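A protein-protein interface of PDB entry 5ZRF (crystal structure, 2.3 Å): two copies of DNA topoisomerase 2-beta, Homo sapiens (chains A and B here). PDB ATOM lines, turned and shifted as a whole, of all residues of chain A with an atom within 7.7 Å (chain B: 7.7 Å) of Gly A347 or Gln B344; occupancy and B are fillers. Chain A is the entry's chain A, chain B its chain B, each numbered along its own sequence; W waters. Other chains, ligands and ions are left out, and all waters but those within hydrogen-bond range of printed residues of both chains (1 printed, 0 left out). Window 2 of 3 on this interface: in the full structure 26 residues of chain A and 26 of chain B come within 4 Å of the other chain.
The side-chain amide nitrogen (NE2) of Gln A344 is in hydrogen-bond range of the backbone carbonyl oxygen (O) of Gln B344 (3.1 Å). The backbone NH (N) of Ser A348 sits close to the side-chain amide nitrogen (NE2) of Gln B344 (3.5 Å). The side-chain carboxylate of Glu A359 lies within salt-bridge range of the side-chain amino group of Lys B341.
The side-chain hydroxyl (OG) of Ser A348 lies within hydrogen-bond range of the guanidinium group (NH1) of Arg A334 (3.0 Å). SD of Met A352 is in hydrogen-bond range of OG of Ser A348 (3.5 Å). OG of Ser B348 is in hydrogen-bond range of NH1 of Arg B334 (2.8 Å). The side-chain amino group (NZ) of Lys B341 sits close to the backbone carbonyl oxygen (O) of Arg B402, at 3.2 Å.
OE1 of Gln A344 touches CA of Gly B347, 3.4 Å away. Ser B348 touches Gln A344 (N to NE2, 3.6 Å). OE1 of Gln B344 touches CA of Gly A347 (3.5 Å).
Of the printed residues of chain B, Gln A344 touches Gln B344, Gly B347 and Ser B348. No residue of chain B comes within 4 Å of Ala A346. Gly A347 touches just one residue of chain B: Gln B344. Of the printed residues of chain B, Ser A348 touches Gln B344. No residue of chain A comes within 4 Å of Ala B343. Gln B344 touches three residues of chain A. Ala B346 touches none of the printed residues of chain A. Printed residues of chain A within 4 Å of Gly B347: Gln A344 (3.4 Å). Of the printed residues of chain A, Ser B348 touches Gln A344. The nearest residue of chain B that does not touch Gly A347 is Lys B341 (5.8 Å).
Printed residues of chain A that touch a printed residue of chain B: Gln A344, Gly A347, Ser A348 and Glu A359.
Gln A344 touches its own counterpart, Gln B344. Gln A344 touches Gly B347, and with the chains exchanged Gly A347 touches Gln B344. Gln A344 touches Ser B348, and with the chains exchanged Ser A348 touches Gln B344. Glu A359 touches Lys B341, but with the chains exchanged Lys A341 does not touch Glu B359 (5.0 Å).
Water W1 lies within hydrogen-bond range of OE2 of Glu A359 (2.8 Å) and NZ of Lys B341 (2.9 Å).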
ATOM      1  N   THR A 330      15.460  -1.450 -15.270  1.00  0.00           N
ATOM      2  CA  THR A 330      15.348  -1.793 -16.685  1.00  0.00           C
ATOM      3  C   THR A 330      16.636  -1.478 -17.439  1.00  0.00           C
ATOM      4  O   THR A 330      17.099  -2.291 -18.245  1.00  0.00           O
ATOM      5  CB  THR A 330      14.162  -1.065 -17.322  1.00  0.00           C
ATOM      6  OG1 THR A 330      12.955  -1.427 -16.637  1.00  0.00           O
ATOM      7  CG2 THR A 330      14.046  -1.447 -18.796  1.00  0.00           C
ATOM      8  N   ARG A 334      18.856  -4.127 -19.462  1.00  0.00           N
ATOM      9  CA  ARG A 334      19.106  -3.941 -20.887  1.00  0.00           C
ATOM     10  C   ARG A 334      20.597  -3.837 -21.176  1.00  0.00           C
ATOM     11  O   ARG A 334      21.078  -4.394 -22.169  1.00  0.00           O
ATOM     12  CB  ARG A 334      18.379  -2.698 -21.396  1.00  0.00           C
ATOM     13  CG  ARG A 334      16.860  -2.784 -21.347  1.00  0.00           C
ATOM     14  CD  ARG A 334      16.265  -1.433 -21.714  1.00  0.00           C
ATOM     15  NE  ARG A 334      16.895  -0.929 -22.929  1.00  0.00           N
ATOM     16  CZ  ARG A 334      16.352  -0.998 -24.142  1.00  0.00           C
ATOM     17  NH1 ARG A 334      15.137  -1.512 -24.301  1.00  0.00           N
ATOM     18  NH2 ARG A 334      17.020  -0.534 -25.193  1.00  0.00           N
ATOM     19  N   VAL A 340      19.497   5.117 -26.490  1.00  0.00           N
ATOM     20  CA  VAL A 340      18.153   4.640 -26.779  1.00  0.00           C
ATOM     21  C   VAL A 340      17.205   5.830 -26.701  1.00  0.00           C
ATOM     22  O   VAL A 340      17.348   6.680 -25.816  1.00  0.00           O
ATOM     23  CB  VAL A 340      17.737   3.536 -25.782  1.00  0.00           C
ATOM     24  CG1 VAL A 340      16.315   3.084 -26.027  1.00  0.00           C
ATOM     25  CG2 VAL A 340      18.703   2.353 -25.865  1.00  0.00           C
ATOM     26  N   LYS A 341      16.238   5.893 -27.621  1.00  0.00           N
ATOM     27  CA  LYS A 341      15.210   6.928 -27.549  1.00  0.00           C
ATOM     28  C   LYS A 341      14.438   6.836 -26.236  1.00  0.00           C
ATOM     29  O   LYS A 341      14.057   5.747 -25.796  1.00  0.00           O
ATOM     30  CB  LYS A 341      14.239   6.810 -28.729  1.00  0.00           C
ATOM     31  CG  LYS A 341      14.350   7.930 -29.750  1.00  0.00           C
ATOM     32  N   VAL A 342      14.192   7.998 -25.623  1.00  0.00           N
ATOM     33  CA  VAL A 342      13.514   8.036 -24.327  1.00  0.00           C
ATOM     34  C   VAL A 342      12.154   7.356 -24.413  1.00  0.00           C
ATOM     35  O   VAL A 342      11.804   6.516 -23.570  1.00  0.00           O
ATOM     36  CB  VAL A 342      13.386   9.488 -23.828  1.00  0.00           C
ATOM     37  CG1 VAL A 342      12.448   9.555 -22.633  1.00  0.00           C
ATOM     38  CG2 VAL A 342      14.755  10.035 -23.460  1.00  0.00           C
ATOM     39  N   ALA A 343      11.366   7.701 -25.438  1.00  0.00           N
ATOM     40  CA  ALA A 343      10.053   7.081 -25.593  1.00  0.00           C
ATOM     41  C   ALA A 343      10.172   5.567 -25.717  1.00  0.00           C
ATOM     42  O   ALA A 343       9.331   4.825 -25.197  1.00  0.00           O
ATOM     43  CB  ALA A 343       9.330   7.669 -26.807  1.00  0.00           C
ATOM     44  N   GLN A 344      11.228   5.096 -26.382  1.00  0.00           N
ATOM     45  CA  GLN A 344      11.443   3.662 -26.530  1.00  0.00           C
ATOM     46  C   GLN A 344      11.871   3.022 -25.209  1.00  0.00           C
ATOM     47  O   GLN A 344      11.380   1.944 -24.852  1.00  0.00           O
ATOM     48  CB  GLN A 344      12.488   3.416 -27.626  1.00  0.00           C
ATOM     49  CG  GLN A 344      12.635   1.981 -28.059  1.00  0.00           C
ATOM     50  CD  GLN A 344      11.476   1.502 -28.915  1.00  0.00           C
ATOM     51  OE1 GLN A 344      10.630   2.293 -29.343  1.00  0.00           O
ATOM     52  NE2 GLN A 344      11.432   0.198 -29.166  1.00  0.00           N
ATOM     53  N   LEU A 345      12.793   3.661 -24.474  1.00  0.00           N
ATOM     54  CA  LEU A 345      13.177   3.124 -23.169  1.00  0.00           C
ATOM     55  C   LEU A 345      11.971   3.037 -22.238  1.00  0.00           C
ATOM     56  O   LEU A 345      11.799   2.044 -21.519  1.00  0.00           O
ATOM     57  CB  LEU A 345      14.282   3.983 -22.546  1.00  0.00           C
ATOM     58  CG  LEU A 345      14.698   3.617 -21.114  1.00  0.00           C
ATOM     59  CD1 LEU A 345      15.108   2.147 -21.023  1.00  0.00           C
ATOM     60  CD2 LEU A 345      15.838   4.497 -20.645  1.00  0.00           C
ATOM     61  N   ALA A 346      11.102   4.051 -22.270  1.00  0.00           N
ATOM     62  CA  ALA A 346       9.917   4.064 -21.416  1.00  0.00           C
ATOM     63  C   ALA A 346       9.018   2.861 -21.683  1.00  0.00           C
ATOM     64  O   ALA A 346       8.541   2.213 -20.745  1.00  0.00           O
ATOM     65  CB  ALA A 346       9.140   5.372 -21.612  1.00  0.00           C
ATOM     66  N   GLY A 347       8.751   2.558 -22.958  1.00  0.00           N
ATOM     67  CA  GLY A 347       7.942   1.385 -23.260  1.00  0.00           C
ATOM     68  C   GLY A 347       8.603   0.100 -22.791  1.00  0.00           C
ATOM     69  O   GLY A 347       7.940  -0.808 -22.277  1.00  0.00           O
ATOM     70  N   SER A 348       9.924   0.024 -22.925  1.00  0.00           N
ATOM     71  CA  SER A 348      10.653  -1.132 -22.409  1.00  0.00           C
ATOM     72  C   SER A 348      10.520  -1.238 -20.888  1.00  0.00           C
ATOM     73  O   SER A 348      10.326  -2.336 -20.350  1.00  0.00           O
ATOM     74  CB  SER A 348      12.118  -1.036 -22.839  1.00  0.00           C
ATOM     75  OG  SER A 348      12.865  -2.133 -22.371  1.00  0.00           O
ATOM     76  N   VAL A 349      10.595  -0.104 -20.180  1.00  0.00           N
ATOM     77  CA  VAL A 349      10.458  -0.130 -18.725  1.00  0.00           C
ATOM     78  C   VAL A 349       9.102  -0.691 -18.324  1.00  0.00           C
ATOM     79  O   VAL A 349       9.001  -1.506 -17.398  1.00  0.00           O
ATOM     80  CB  VAL A 349      10.679   1.273 -18.134  1.00  0.00           C
ATOM     81  CG1 VAL A 349      10.379   1.268 -16.638  1.00  0.00           C
ATOM     82  CG2 VAL A 349      12.109   1.739 -18.384  1.00  0.00           C
ATOM     83  N   ALA A 350       8.038  -0.271 -19.016  1.00  0.00           N
ATOM     84  CA  ALA A 350       6.702  -0.745 -18.665  1.00  0.00           C
ATOM     85  C   ALA A 350       6.590  -2.249 -18.863  1.00  0.00           C
ATOM     86  O   ALA A 350       6.069  -2.964 -18.001  1.00  0.00           O
ATOM     87  CB  ALA A 350       5.641  -0.010 -19.489  1.00  0.00           C
ATOM     88  N   GLU A 351       7.088  -2.750 -19.994  1.00  0.00           N
ATOM     89  CA  GLU A 351       7.089  -4.190 -20.230  1.00  0.00           C
ATOM     90  C   GLU A 351       7.904  -4.924 -19.168  1.00  0.00           C
ATOM     91  O   GLU A 351       7.410  -5.853 -18.518  1.00  0.00           O
ATOM     92  CB  GLU A 351       7.639  -4.488 -21.627  1.00  0.00           C
ATOM     93  N   MET A 352       9.156  -4.509 -18.965  1.00  0.00           N
ATOM     94  CA  MET A 352      10.070  -5.303 -18.148  1.00  0.00           C
ATOM     95  C   MET A 352       9.809  -5.163 -16.651  1.00  0.00           C
ATOM     96  O   MET A 352      10.001  -6.124 -15.900  1.00  0.00           O
ATOM     97  CB  MET A 352      11.519  -4.940 -18.479  1.00  0.00           C
ATOM     98  CG  MET A 352      11.958  -5.516 -19.823  1.00  0.00           C
ATOM     99  SD  MET A 352      13.585  -5.008 -20.434  1.00  0.00           S
ATOM    100  CE  MET A 352      14.556  -5.258 -18.970  1.00  0.00           C
ATOM    101  N   SER A 353       9.443  -3.973 -16.184  1.00  0.00           N
ATOM    102  CA  SER A 353       9.250  -3.746 -14.759  1.00  0.00           C
ATOM    103  C   SER A 353       7.793  -3.771 -14.304  1.00  0.00           C
ATOM    104  O   SER A 353       7.538  -3.585 -13.110  1.00  0.00           O
ATOM    105  CB  SER A 353       9.889  -2.420 -14.360  1.00  0.00           C
ATOM    106  OG  SER A 353       9.074  -1.332 -14.763  1.00  0.00           O
ATOM    107  N   TYR A 355       5.372  -1.492 -14.992  1.00  0.00           N
ATOM    108  CA  TYR A 355       4.923  -0.155 -14.624  1.00  0.00           C
ATOM    109  C   TYR A 355       3.482   0.028 -15.094  1.00  0.00           C
ATOM    110  O   TYR A 355       3.184  -0.144 -16.278  1.00  0.00           O
ATOM    111  CB  TYR A 355       5.844   0.893 -15.241  1.00  0.00           C
ATOM    112  CG  TYR A 355       5.492   2.341 -14.933  1.00  0.00           C
ATOM    113  CD1 TYR A 355       5.904   2.948 -13.743  1.00  0.00           C
ATOM    114  CD2 TYR A 355       4.786   3.106 -15.845  1.00  0.00           C
ATOM    115  CE1 TYR A 355       5.602   4.270 -13.474  1.00  0.00           C
ATOM    116  CE2 TYR A 355       4.478   4.426 -15.585  1.00  0.00           C
ATOM    117  CZ  TYR A 355       4.893   5.003 -14.404  1.00  0.00           C
ATOM    118  OH  TYR A 355       4.591   6.317 -14.168  1.00  0.00           O
ATOM    119  N   GLU A 359       2.714   6.041 -19.805  1.00  0.00           N
ATOM    120  CA  GLU A 359       4.124   6.127 -20.176  1.00  0.00           C
ATOM    121  C   GLU A 359       4.614   7.562 -20.266  1.00  0.00           C
ATOM    122  O   GLU A 359       5.811   7.811 -20.077  1.00  0.00           O
ATOM    123  CB  GLU A 359       4.365   5.422 -21.506  1.00  0.00           C
ATOM    124  CG  GLU A 359       3.901   3.998 -21.493  1.00  0.00           C
ATOM    125  CD  GLU A 359       4.522   3.186 -22.594  1.00  0.00           C
ATOM    126  OE1 GLU A 359       5.010   3.784 -23.581  1.00  0.00           O
ATOM    127  OE2 GLU A 359       4.519   1.949 -22.460  1.00  0.00           O
ATOM    128  N   LEU A 362       6.317   8.200 -17.192  1.00  0.00           N
ATOM    129  CA  LEU A 362       7.627   7.561 -17.172  1.00  0.00           C
ATOM    130  C   LEU A 362       8.637   8.352 -17.986  1.00  0.00           C
ATOM    131  O   LEU A 362       9.794   8.511 -17.573  1.00  0.00           O
ATOM    132  CB  LEU A 362       7.532   6.142 -17.721  1.00  0.00           C
ATOM    133  CG  LEU A 362       7.665   4.945 -16.792  1.00  0.00           C
ATOM    134  CD1 LEU A 362       7.906   3.701 -17.647  1.00  0.00           C
ATOM    135  CD2 LEU A 362       8.764   5.138 -15.749  1.00  0.00           C
ATOM    136  N   MET A 363       8.225   8.836 -19.160  1.00  0.00           N
ATOM    137  CA  MET A 363       9.137   9.623 -19.985  1.00  0.00           C
ATOM    138  C   MET A 363       9.602  10.882 -19.253  1.00  0.00           C
ATOM    139  O   MET A 363      10.783  11.250 -19.327  1.00  0.00           O
ATOM    140  CB  MET A 363       8.472   9.965 -21.319  1.00  0.00           C
ATOM    141  CG  MET A 363       8.273   8.754 -22.244  1.00  0.00           C
ATOM    142  SD  MET A 363       7.292   9.124 -23.712  1.00  0.00           S
ATOM    143  CE  MET A 363       6.605   7.515 -24.081  1.00  0.00           C
ATOM    144  N   ILE A 366      12.223   9.789 -16.753  1.00  0.00           N
ATOM    145  CA  ILE A 366      13.510   9.530 -17.401  1.00  0.00           C
ATOM    146  C   ILE A 366      14.232  10.837 -17.710  1.00  0.00           C
ATOM    147  O   ILE A 366      15.446  10.954 -17.506  1.00  0.00           O
ATOM    148  CB  ILE A 366      13.308   8.694 -18.676  1.00  0.00           C
ATOM    149  CG1 ILE A 366      12.866   7.277 -18.312  1.00  0.00           C
ATOM    150  CG2 ILE A 366      14.583   8.706 -19.526  1.00  0.00           C
ATOM    151  CD1 ILE A 366      12.220   6.537 -19.473  1.00  0.00           C
ATOM    152  N   THR B 330      11.354  -5.654 -40.006  1.00  0.00           N
ATOM    153  CA  THR B 330      11.642  -5.563 -38.578  1.00  0.00           C
ATOM    154  C   THR B 330      10.918  -6.653 -37.800  1.00  0.00           C
ATOM    155  O   THR B 330      11.508  -7.286 -36.917  1.00  0.00           O
ATOM    156  CB  THR B 330      11.251  -4.187 -38.042  1.00  0.00           C
ATOM    157  OG1 THR B 330      11.850  -3.166 -38.848  1.00  0.00           O
ATOM    158  CG2 THR B 330      11.722  -4.015 -36.600  1.00  0.00           C
ATOM    159  N   ARG B 334      12.652  -9.358 -35.365  1.00  0.00           N
ATOM    160  CA  ARG B 334      12.341  -9.487 -33.942  1.00  0.00           C
ATOM    161  C   ARG B 334      11.742 -10.852 -33.619  1.00  0.00           C
ATOM    162  O   ARG B 334      12.077 -11.450 -32.591  1.00  0.00           O
ATOM    163  CB  ARG B 334      11.386  -8.378 -33.493  1.00  0.00           C
ATOM    164  CG  ARG B 334      11.829  -6.966 -33.851  1.00  0.00           C
ATOM    165  CD  ARG B 334      10.744  -5.949 -33.556  1.00  0.00           C
ATOM    166  NE  ARG B 334      10.038  -6.268 -32.315  1.00  0.00           N
ATOM    167  CZ  ARG B 334      10.207  -5.622 -31.159  1.00  0.00           C
ATOM    168  NH1 ARG B 334      11.055  -4.603 -31.071  1.00  0.00           N
ATOM    169  NH2 ARG B 334       9.519  -5.990 -30.086  1.00  0.00           N
ATOM    170  N   VAL B 340       3.222  -6.528 -28.993  1.00  0.00           N
ATOM    171  CA  VAL B 340       4.089  -5.370 -28.815  1.00  0.00           C
ATOM    172  C   VAL B 340       3.257  -4.113 -29.046  1.00  0.00           C
ATOM    173  O   VAL B 340       2.445  -4.062 -29.977  1.00  0.00           O
ATOM    174  CB  VAL B 340       5.295  -5.415 -29.781  1.00  0.00           C
ATOM    175  CG1 VAL B 340       6.234  -4.252 -29.532  1.00  0.00           C
ATOM    176  CG2 VAL B 340       6.042  -6.741 -29.646  1.00  0.00           C
ATOM    177  N   LYS B 341       3.445  -3.111 -28.187  1.00  0.00           N
ATOM    178  CA  LYS B 341       2.817  -1.811 -28.400  1.00  0.00           C
ATOM    179  C   LYS B 341       3.202  -1.262 -29.766  1.00  0.00           C
ATOM    180  O   LYS B 341       4.370  -1.302 -30.155  1.00  0.00           O
ATOM    181  CB  LYS B 341       3.259  -0.818 -27.324  1.00  0.00           C
ATOM    182  CG  LYS B 341       2.759  -1.107 -25.935  1.00  0.00           C
ATOM    183  CD  LYS B 341       1.400  -0.482 -25.716  1.00  0.00           C
ATOM    184  CE  LYS B 341       1.241  -0.078 -24.261  1.00  0.00           C
ATOM    185  NZ  LYS B 341       2.199   1.001 -23.897  1.00  0.00           N
ATOM    186  N   VAL B 342       2.224  -0.714 -30.486  1.00  0.00           N
ATOM    187  CA  VAL B 342       2.514  -0.215 -31.828  1.00  0.00           C
ATOM    188  C   VAL B 342       3.546   0.907 -31.765  1.00  0.00           C
ATOM    189  O   VAL B 342       4.458   0.975 -32.599  1.00  0.00           O
ATOM    190  CB  VAL B 342       1.221   0.233 -32.537  1.00  0.00           C
ATOM    191  CG1 VAL B 342       1.547   1.036 -33.791  1.00  0.00           C
ATOM    192  CG2 VAL B 342       0.345  -0.966 -32.874  1.00  0.00           C
ATOM    193  N   ALA B 343       3.435   1.792 -30.767  1.00  0.00           N
ATOM    194  CA  ALA B 343       4.415   2.868 -30.630  1.00  0.00           C
ATOM    195  C   ALA B 343       5.805   2.307 -30.379  1.00  0.00           C
ATOM    196  O   ALA B 343       6.798   2.807 -30.923  1.00  0.00           O
ATOM    197  CB  ALA B 343       4.014   3.819 -29.501  1.00  0.00           C
ATOM    198  N   GLN B 344       5.890   1.243 -29.582  1.00  0.00           N
ATOM    199  CA  GLN B 344       7.171   0.590 -29.343  1.00  0.00           C
ATOM    200  C   GLN B 344       7.694  -0.082 -30.609  1.00  0.00           C
ATOM    201  O   GLN B 344       8.881   0.033 -30.936  1.00  0.00           O
ATOM    202  CB  GLN B 344       7.016  -0.418 -28.204  1.00  0.00           C
ATOM    203  CG  GLN B 344       8.312  -1.023 -27.704  1.00  0.00           C
ATOM    204  CD  GLN B 344       9.113  -0.067 -26.848  1.00  0.00           C
ATOM    205  OE1 GLN B 344       8.726   1.090 -26.650  1.00  0.00           O
ATOM    206  NE2 GLN B 344      10.239  -0.548 -26.327  1.00  0.00           N
ATOM    207  N   LEU B 345       6.829  -0.788 -31.337  1.00  0.00           N
ATOM    208  CA  LEU B 345       7.265  -1.402 -32.587  1.00  0.00           C
ATOM    209  C   LEU B 345       7.778  -0.348 -33.562  1.00  0.00           C
ATOM    210  O   LEU B 345       8.818  -0.539 -34.202  1.00  0.00           O
ATOM    211  CB  LEU B 345       6.120  -2.204 -33.212  1.00  0.00           C
ATOM    212  CG  LEU B 345       6.447  -2.978 -34.498  1.00  0.00           C
ATOM    213  CD1 LEU B 345       7.645  -3.880 -34.296  1.00  0.00           C
ATOM    214  CD2 LEU B 345       5.264  -3.779 -34.967  1.00  0.00           C
ATOM    215  N   ALA B 346       7.085   0.789 -33.658  1.00  0.00           N
ATOM    216  CA  ALA B 346       7.495   1.831 -34.598  1.00  0.00           C
ATOM    217  C   ALA B 346       8.918   2.309 -34.320  1.00  0.00           C
ATOM    218  O   ALA B 346       9.728   2.457 -35.245  1.00  0.00           O
ATOM    219  CB  ALA B 346       6.511   2.999 -34.539  1.00  0.00           C
ATOM    220  N   GLY B 347       9.249   2.549 -33.048  1.00  0.00           N
ATOM    221  CA  GLY B 347      10.610   2.953 -32.718  1.00  0.00           C
ATOM    222  C   GLY B 347      11.622   1.859 -33.001  1.00  0.00           C
ATOM    223  O   GLY B 347      12.751   2.128 -33.420  1.00  0.00           O
ATOM    224  N   SER B 348      11.232   0.608 -32.768  1.00  0.00           N
ATOM    225  CA  SER B 348      12.085  -0.511 -33.139  1.00  0.00           C
ATOM    226  C   SER B 348      12.308  -0.555 -34.652  1.00  0.00           C
ATOM    227  O   SER B 348      13.436  -0.771 -35.113  1.00  0.00           O
ATOM    228  CB  SER B 348      11.456  -1.812 -32.629  1.00  0.00           C
ATOM    229  OG  SER B 348      12.231  -2.947 -32.958  1.00  0.00           O
ATOM    230  N   VAL B 349      11.250  -0.332 -35.439  1.00  0.00           N
ATOM    231  CA  VAL B 349      11.384  -0.325 -36.897  1.00  0.00           C
ATOM    232  C   VAL B 349      12.336   0.780 -37.340  1.00  0.00           C
ATOM    233  O   VAL B 349      13.196   0.571 -38.205  1.00  0.00           O
ATOM    234  CB  VAL B 349      10.008  -0.168 -37.570  1.00  0.00           C
ATOM    235  CG1 VAL B 349      10.177  -0.032 -39.096  1.00  0.00           C
ATOM    236  CG2 VAL B 349       9.104  -1.354 -37.236  1.00  0.00           C
ATOM    237  N   ALA B 350      12.180   1.980 -36.768  1.00  0.00           N
ATOM    238  CA  ALA B 350      13.023   3.103 -37.165  1.00  0.00           C
ATOM    239  C   ALA B 350      14.494   2.787 -36.945  1.00  0.00           C
ATOM    240  O   ALA B 350      15.335   3.047 -37.814  1.00  0.00           O
ATOM    241  CB  ALA B 350      12.624   4.361 -36.388  1.00  0.00           C
ATOM    242  N   GLU B 351      14.821   2.212 -35.794  1.00  0.00           N
ATOM    243  CA  GLU B 351      16.208   1.880 -35.504  1.00  0.00           C
ATOM    244  C   GLU B 351      16.709   0.734 -36.387  1.00  0.00           C
ATOM    245  O   GLU B 351      17.791   0.829 -36.978  1.00  0.00           O
ATOM    246  CB  GLU B 351      16.328   1.553 -34.015  1.00  0.00           C
ATOM    247  CG  GLU B 351      17.461   0.654 -33.617  1.00  0.00           C
ATOM    248  CD  GLU B 351      17.524   0.463 -32.109  1.00  0.00           C
ATOM    249  OE1 GLU B 351      16.479   0.654 -31.441  1.00  0.00           O
ATOM    250  OE2 GLU B 351      18.613   0.127 -31.593  1.00  0.00           O
ATOM    251  N   GLU B 359       8.066   9.070 -36.824  1.00  0.00           N
ATOM    252  CA  GLU B 359       7.564   7.786 -36.353  1.00  0.00           C
ATOM    253  C   GLU B 359       6.045   7.727 -36.324  1.00  0.00           C
ATOM    254  O   GLU B 359       5.484   6.627 -36.401  1.00  0.00           O
ATOM    255  CB  GLU B 359       8.135   7.465 -34.971  1.00  0.00           C
ATOM    256  CG  GLU B 359       9.566   6.926 -35.040  1.00  0.00           C
ATOM    257  CD  GLU B 359      10.137   6.543 -33.681  1.00  0.00           C
ATOM    258  OE1 GLU B 359       9.348   6.316 -32.736  1.00  0.00           O
ATOM    259  OE2 GLU B 359      11.380   6.482 -33.560  1.00  0.00           O
ATOM    260  N   MET B 363       3.610   4.621 -37.346  1.00  0.00           N
ATOM    261  CA  MET B 363       2.557   4.046 -36.513  1.00  0.00           C
ATOM    262  C   MET B 363       1.241   3.927 -37.276  1.00  0.00           C
ATOM    263  O   MET B 363       0.526   2.924 -37.143  1.00  0.00           O
ATOM    264  CB  MET B 363       2.371   4.896 -35.260  1.00  0.00           C
ATOM    265  CG  MET B 363       3.608   4.948 -34.397  1.00  0.00           C
ATOM    266  SD  MET B 363       3.404   5.974 -32.935  1.00  0.00           S
ATOM    267  CE  MET B 363       5.085   5.980 -32.329  1.00  0.00           C
ATOM    268  N   ILE B 366       1.600   1.065 -39.470  1.00  0.00           N
ATOM    269  CA  ILE B 366       1.440  -0.178 -38.717  1.00  0.00           C
ATOM    270  C   ILE B 366      -0.036  -0.450 -38.426  1.00  0.00           C
ATOM    271  O   ILE B 366      -0.512  -1.576 -38.598  1.00  0.00           O
ATOM    272  CB  ILE B 366       2.292  -0.135 -37.434  1.00  0.00           C
ATOM    273  CG1 ILE B 366       3.780  -0.164 -37.799  1.00  0.00           C
ATOM    274  CG2 ILE B 366       1.934  -1.291 -36.505  1.00  0.00           C
ATOM    275  CD1 ILE B 366       4.708   0.262 -36.668  1.00  0.00           C
ATOM    276  N   PRO B 401      -1.816   4.790 -30.931  1.00  0.00           N
ATOM    277  CA  PRO B 401      -0.774   3.756 -31.069  1.00  0.00           C
ATOM    278  C   PRO B 401      -0.028   3.489 -29.774  1.00  0.00           C
ATOM    279  O   PRO B 401       0.697   2.493 -29.682  1.00  0.00           O
ATOM    280  CB  PRO B 401       0.151   4.322 -32.157  1.00  0.00           C
ATOM    281  CG  PRO B 401      -0.128   5.785 -32.182  1.00  0.00           C
ATOM    282  CD  PRO B 401      -1.559   5.966 -31.779  1.00  0.00           C
ATOM    283  N   ARG B 402      -0.155   4.370 -28.782  1.00  0.00           N
ATOM    284  CA  ARG B 402       0.404   4.090 -27.465  1.00  0.00           C
ATOM    285  C   ARG B 402      -0.426   3.062 -26.698  1.00  0.00           C
ATOM    286  O   ARG B 402       0.064   2.483 -25.724  1.00  0.00           O
ATOM    287  CB  ARG B 402       0.504   5.391 -26.654  1.00  0.00           C
ATOM    288  CG  ARG B 402       1.460   6.441 -27.223  1.00  0.00           C
ATOM    289  CD  ARG B 402       1.447   7.753 -26.413  1.00  0.00           C
ATOM    290  NE  ARG B 402       0.593   8.775 -27.018  1.00  0.00           N
ATOM    291  CZ  ARG B 402      -0.594   9.146 -26.542  1.00  0.00           C
ATOM    292  NH1 ARG B 402      -1.072   8.590 -25.437  1.00  0.00           N
ATOM    293  NH2 ARG B 402      -1.301  10.084 -27.166  1.00  0.00           N
ATOM    294  N   ILE B 404      -2.334   0.412 -28.153  1.00  0.00           N
ATOM    295  CA  ILE B 404      -2.725  -0.785 -28.885  1.00  0.00           C
ATOM    296  C   ILE B 404      -1.486  -1.611 -29.198  1.00  0.00           C
ATOM    297  O   ILE B 404      -0.360  -1.111 -29.220  1.00  0.00           O
ATOM    298  CB  ILE B 404      -3.519  -0.456 -30.169  1.00  0.00           C
ATOM    299  CG1 ILE B 404      -2.666   0.361 -31.145  1.00  0.00           C
ATOM    300  CG2 ILE B 404      -4.785   0.302 -29.816  1.00  0.00           C
ATOM    301  CD1 ILE B 404      -3.441   0.895 -32.335  1.00  0.00           C
HETATM  302  O   HOH W   1       2.488   0.738 -21.013  1.00  0.00           O
